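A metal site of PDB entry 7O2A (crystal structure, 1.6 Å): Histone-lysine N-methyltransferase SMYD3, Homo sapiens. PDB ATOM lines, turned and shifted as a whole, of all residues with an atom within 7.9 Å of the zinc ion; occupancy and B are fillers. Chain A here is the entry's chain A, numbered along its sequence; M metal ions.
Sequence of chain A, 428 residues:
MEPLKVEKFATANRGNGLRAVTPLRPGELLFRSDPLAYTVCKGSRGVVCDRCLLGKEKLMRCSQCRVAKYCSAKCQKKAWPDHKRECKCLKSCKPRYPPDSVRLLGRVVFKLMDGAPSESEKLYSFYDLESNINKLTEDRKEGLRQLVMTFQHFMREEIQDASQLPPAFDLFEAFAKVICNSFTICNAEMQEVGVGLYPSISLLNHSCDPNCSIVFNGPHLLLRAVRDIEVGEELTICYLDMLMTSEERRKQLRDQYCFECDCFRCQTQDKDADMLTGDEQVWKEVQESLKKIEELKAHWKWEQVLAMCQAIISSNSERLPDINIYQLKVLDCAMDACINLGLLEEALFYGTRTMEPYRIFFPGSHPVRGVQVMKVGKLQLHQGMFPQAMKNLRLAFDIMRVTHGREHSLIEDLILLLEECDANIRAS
N of Leu 54 lies close to SG of Cys 52, 3.7 Å away.
N of Arg 51 lies close to SG of Cys 49 (3.5 Å).
The backbone carbonyl oxygen (O) of Leu 54 sits at hydrogen-bond distance from the backbone NH (N) of Cys 49, 2.8 Å away.
The backbone NH (N) of Cys 75 is in hydrogen-bond range of the side-chain hydroxyl (OG) of Ser 72, at 3.1 Å.
The side-chain sulfur (SG) of Cys 71 sits close to the side-chain hydroxyl (OG) of Ser 72, 3.3 Å away.
Four residues have an atom within 4 Å of the zinc ion: Cys 49, Cys 52, Cys 71 and Cys 75.
The zinc ion is bound by the side-chain sulfur (SG) of Cys 71.
SG of Cys 75 binds the zinc ion, at 2.3 Å.
SG of Cys 52 binds the zinc ion, 2.3 Å away.
SG of Cys 49 binds the zinc ion (2.3 Å).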
ATOM      1  N   VAL A  48      -2.516 -11.207   3.619  1.00  0.00           N
ATOM      2  CA  VAL A  48      -2.907 -11.667   4.938  1.00  0.00           C
ATOM      3  C   VAL A  48      -2.236 -10.854   6.005  1.00  0.00           C
ATOM      4  O   VAL A  48      -1.211 -10.246   5.761  1.00  0.00           O
ATOM      5  CB  VAL A  48      -2.605 -13.176   5.164  1.00  0.00           C
ATOM      6  CG1 VAL A  48      -3.326 -14.046   4.140  1.00  0.00           C
ATOM      7  CG2 VAL A  48      -1.123 -13.452   5.199  1.00  0.00           C
ATOM      8  N   CYS A  49      -2.810 -10.905   7.213  1.00  0.00           N
ATOM      9  CA  CYS A  49      -2.301 -10.137   8.323  1.00  0.00           C
ATOM     10  C   CYS A  49      -0.894 -10.641   8.673  1.00  0.00           C
ATOM     11  O   CYS A  49      -0.698 -11.848   8.902  1.00  0.00           O
ATOM     12  CB  CYS A  49      -3.278 -10.291   9.507  1.00  0.00           C
ATOM     13  SG  CYS A  49      -2.780  -9.418  11.033  1.00  0.00           S
ATOM     14  N   ASP A  50       0.110  -9.726   8.772  1.00  0.00           N
ATOM     15  CA  ASP A  50       1.450 -10.101   9.281  1.00  0.00           C
ATOM     16  C   ASP A  50       1.441 -10.859  10.565  1.00  0.00           C
ATOM     17  O   ASP A  50       2.265 -11.789  10.738  1.00  0.00           O
ATOM     18  CB  ASP A  50       2.257  -8.847   9.556  1.00  0.00           C
ATOM     19  CG  ASP A  50       3.150  -8.439   8.396  1.00  0.00           C
ATOM     20  OD1 ASP A  50       2.708  -8.346   7.229  1.00  0.00           O
ATOM     21  OD2 ASP A  50       4.346  -8.226   8.664  1.00  0.00           O
ATOM     22  N   ARG A  51       0.544 -10.556  11.485  1.00  0.00           N
ATOM     23  CA  ARG A  51       0.564 -11.202  12.787  1.00  0.00           C
ATOM     24  C   ARG A  51      -0.243 -12.505  12.751  1.00  0.00           C
ATOM     25  O   ARG A  51       0.299 -13.553  13.021  1.00  0.00           O
ATOM     26  CB  ARG A  51       0.067 -10.270  13.934  1.00  0.00           C
ATOM     27  CG  ARG A  51       0.117 -10.976  15.287  1.00  0.00           C
ATOM     28  CD  ARG A  51       0.553 -10.126  16.453  1.00  0.00           C
ATOM     29  NE  ARG A  51       0.531 -10.845  17.727  1.00  0.00           N
ATOM     30  CZ  ARG A  51       1.590 -11.368  18.333  1.00  0.00           C
ATOM     31  NH1 ARG A  51       2.758 -11.269  17.790  1.00  0.00           N
ATOM     32  NH2 ARG A  51       1.441 -11.973  19.479  1.00  0.00           N
ATOM     33  N   CYS A  52      -1.550 -12.446  12.462  1.00  0.00           N
ATOM     34  CA  CYS A  52      -2.381 -13.649  12.670  1.00  0.00           C
ATOM     35  C   CYS A  52      -2.470 -14.547  11.415  1.00  0.00           C
ATOM     36  O   CYS A  52      -3.066 -15.635  11.500  1.00  0.00           O
ATOM     37  CB  CYS A  52      -3.806 -13.297  13.207  1.00  0.00           C
ATOM     38  SG  CYS A  52      -4.818 -12.399  12.039  1.00  0.00           S
ATOM     39  N   LEU A  53      -1.999 -14.045  10.256  1.00  0.00           N
ATOM     40  CA  LEU A  53      -1.979 -14.782   8.979  1.00  0.00           C
ATOM     41  C   LEU A  53      -3.364 -15.121   8.404  1.00  0.00           C
ATOM     42  O   LEU A  53      -3.467 -16.025   7.570  1.00  0.00           O
ATOM     43  CB  LEU A  53      -1.059 -16.042   9.076  1.00  0.00           C
ATOM     44  CG  LEU A  53       0.355 -15.822   9.669  1.00  0.00           C
ATOM     45  CD1 LEU A  53       1.130 -17.144   9.759  1.00  0.00           C
ATOM     46  CD2 LEU A  53       1.117 -14.813   8.813  1.00  0.00           C
ATOM     47  N   LEU A  54      -4.383 -14.392   8.908  1.00  0.00           N
ATOM     48  CA  LEU A  54      -5.756 -14.409   8.338  1.00  0.00           C
ATOM     49  C   LEU A  54      -5.902 -13.349   7.253  1.00  0.00           C
ATOM     50  O   LEU A  54      -5.290 -12.296   7.329  1.00  0.00           O
ATOM     51  CB  LEU A  54      -6.802 -14.215   9.430  1.00  0.00           C
ATOM     52  CG  LEU A  54      -6.703 -15.171  10.605  1.00  0.00           C
ATOM     53  CD1 LEU A  54      -7.718 -14.926  11.742  1.00  0.00           C
ATOM     54  CD2 LEU A  54      -6.761 -16.603  10.044  1.00  0.00           C
ATOM     55  N   GLY A  55      -6.642 -13.656   6.160  1.00  0.00           N
ATOM     56  CA  GLY A  55      -6.944 -12.680   5.086  1.00  0.00           C
ATOM     57  C   GLY A  55      -8.067 -11.717   5.529  1.00  0.00           C
ATOM     58  O   GLY A  55      -8.728 -11.929   6.531  1.00  0.00           O
ATOM     59  N   LYS A  56      -8.191 -10.590   4.862  1.00  0.00           N
ATOM     60  CA  LYS A  56      -9.296  -9.649   5.144  1.00  0.00           C
ATOM     61  C   LYS A  56      -9.525  -8.773   3.932  1.00  0.00           C
ATOM     62  O   LYS A  56      -8.599  -8.606   3.126  1.00  0.00           O
ATOM     63  CB  LYS A  56      -9.009  -8.742   6.339  1.00  0.00           C
ATOM     64  CG  LYS A  56      -9.637  -9.223   7.634  1.00  0.00           C
ATOM     65  CD  LYS A  56     -10.360  -8.126   8.394  1.00  0.00           C
ATOM     66  CE  LYS A  56     -11.150  -8.775   9.524  1.00  0.00           C
ATOM     67  NZ  LYS A  56     -11.983  -7.829  10.307  1.00  0.00           N
ATOM     68  N   LEU A  59      -6.695  -4.569   4.647  1.00  0.00           N
ATOM     69  CA  LEU A  59      -5.603  -4.549   5.591  1.00  0.00           C
ATOM     70  C   LEU A  59      -4.983  -3.148   5.794  1.00  0.00           C
ATOM     71  O   LEU A  59      -4.755  -2.392   4.844  1.00  0.00           O
ATOM     72  CB  LEU A  59      -4.498  -5.503   5.117  1.00  0.00           C
ATOM     73  CG  LEU A  59      -4.916  -6.962   5.042  1.00  0.00           C
ATOM     74  CD1 LEU A  59      -3.770  -7.716   4.409  1.00  0.00           C
ATOM     75  CD2 LEU A  59      -5.308  -7.564   6.386  1.00  0.00           C
ATOM     76  N   LYS A  69       1.493  -5.295   7.200  1.00  0.00           N
ATOM     77  CA  LYS A  69       0.074  -4.982   7.123  1.00  0.00           C
ATOM     78  C   LYS A  69      -0.714  -5.874   8.042  1.00  0.00           C
ATOM     79  O   LYS A  69      -0.280  -7.002   8.338  1.00  0.00           O
ATOM     80  CB  LYS A  69      -0.478  -5.080   5.706  1.00  0.00           C
ATOM     81  CG  LYS A  69       0.347  -4.254   4.767  1.00  0.00           C
ATOM     82  CD  LYS A  69      -0.195  -4.121   3.371  1.00  0.00           C
ATOM     83  CE  LYS A  69       0.627  -3.090   2.592  1.00  0.00           C
ATOM     84  NZ  LYS A  69       0.670  -3.377   1.136  1.00  0.00           N
ATOM     85  N   TYR A  70      -1.827  -5.374   8.556  1.00  0.00           N
ATOM     86  CA  TYR A  70      -2.482  -6.031   9.660  1.00  0.00           C
ATOM     87  C   TYR A  70      -3.969  -6.022   9.502  1.00  0.00           C
ATOM     88  O   TYR A  70      -4.573  -5.166   8.805  1.00  0.00           O
ATOM     89  CB  TYR A  70      -2.171  -5.307  10.959  1.00  0.00           C
ATOM     90  CG  TYR A  70      -0.698  -5.271  11.228  1.00  0.00           C
ATOM     91  CD1 TYR A  70      -0.056  -6.389  11.756  1.00  0.00           C
ATOM     92  CD2 TYR A  70       0.066  -4.131  10.931  1.00  0.00           C
ATOM     93  CE1 TYR A  70       1.316  -6.362  12.025  1.00  0.00           C
ATOM     94  CE2 TYR A  70       1.426  -4.105  11.218  1.00  0.00           C
ATOM     95  CZ  TYR A  70       2.042  -5.234  11.713  1.00  0.00           C
ATOM     96  OH  TYR A  70       3.390  -5.241  12.048  1.00  0.00           O
ATOM     97  N   CYS A  71      -4.616  -6.974  10.171  1.00  0.00           N
ATOM     98  CA  CYS A  71      -6.061  -7.102  10.002  1.00  0.00           C
ATOM     99  C   CYS A  71      -6.815  -6.112  10.865  1.00  0.00           C
ATOM    100  O   CYS A  71      -7.979  -5.881  10.619  1.00  0.00           O
ATOM    101  CB  CYS A  71      -6.555  -8.491  10.325  1.00  0.00           C
ATOM    102  SG  CYS A  71      -6.448  -9.062  11.991  1.00  0.00           S
ATOM    103  N   SER A  72      -6.179  -5.602  11.916  1.00  0.00           N
ATOM    104  CA  SER A  72      -6.848  -4.943  12.995  1.00  0.00           C
ATOM    105  C   SER A  72      -5.856  -4.123  13.782  1.00  0.00           C
ATOM    106  O   SER A  72      -4.644  -4.391  13.781  1.00  0.00           O
ATOM    107  CB  SER A  72      -7.498  -5.945  13.933  1.00  0.00           C
ATOM    108  OG  SER A  72      -6.509  -6.894  14.483  1.00  0.00           O
ATOM    109  N   ALA A  73      -6.383  -3.117  14.478  1.00  0.00           N
ATOM    110  CA  ALA A  73      -5.534  -2.386  15.449  1.00  0.00           C
ATOM    111  C   ALA A  73      -4.879  -3.340  16.498  1.00  0.00           C
ATOM    112  O   ALA A  73      -3.702  -3.173  16.884  1.00  0.00           O
ATOM    113  CB  ALA A  73      -6.368  -1.336  16.145  1.00  0.00           C
ATOM    114  N   LYS A  74      -5.603  -4.322  16.967  1.00  0.00           N
ATOM    115  CA  LYS A  74      -5.117  -5.229  17.962  1.00  0.00           C
ATOM    116  C   LYS A  74      -3.880  -5.968  17.409  1.00  0.00           C
ATOM    117  O   LYS A  74      -2.862  -6.065  18.080  1.00  0.00           O
ATOM    118  CB  LYS A  74      -6.188  -6.240  18.395  1.00  0.00           C
ATOM    119  CG  LYS A  74      -5.619  -7.424  19.195  1.00  0.00           C
ATOM    120  CD  LYS A  74      -6.651  -8.397  19.805  1.00  0.00           C
ATOM    121  CE  LYS A  74      -5.921  -9.206  20.899  1.00  0.00           C
ATOM    122  NZ  LYS A  74      -6.750 -10.357  21.340  1.00  0.00           N
ATOM    123  N   CYS A  75      -3.987  -6.457  16.191  1.00  0.00           N
ATOM    124  CA  CYS A  75      -2.818  -7.170  15.592  1.00  0.00           C
ATOM    125  C   CYS A  75      -1.629  -6.316  15.315  1.00  0.00           C
ATOM    126  O   CYS A  75      -0.476  -6.709  15.593  1.00  0.00           O
ATOM    127  CB  CYS A  75      -3.169  -7.918  14.308  1.00  0.00           C
ATOM    128  SG  CYS A  75      -3.982  -9.544  14.579  1.00  0.00           S
ATOM    129  N   GLN A  76      -1.892  -5.097  14.848  1.00  0.00           N
ATOM    130  CA  GLN A  76      -0.761  -4.168  14.589  1.00  0.00           C
ATOM    131  C   GLN A  76      -0.046  -3.841  15.901  1.00  0.00           C
ATOM    132  O   GLN A  76       1.186  -3.829  15.974  1.00  0.00           O
ATOM    133  CB  GLN A  76      -1.300  -2.894  13.906  1.00  0.00           C
ATOM    134  CG  GLN A  76      -0.200  -1.938  13.635  1.00  0.00           C
ATOM    135  CD  GLN A  76      -0.560  -0.811  12.712  1.00  0.00           C
ATOM    136  OE1 GLN A  76      -1.649  -0.782  12.092  1.00  0.00           O
ATOM    137  NE2 GLN A  76       0.348   0.105  12.570  1.00  0.00           N
HETATM  138 ZN    ZN M   1      -4.508 -10.157  12.438  1.00  0.00          ZN
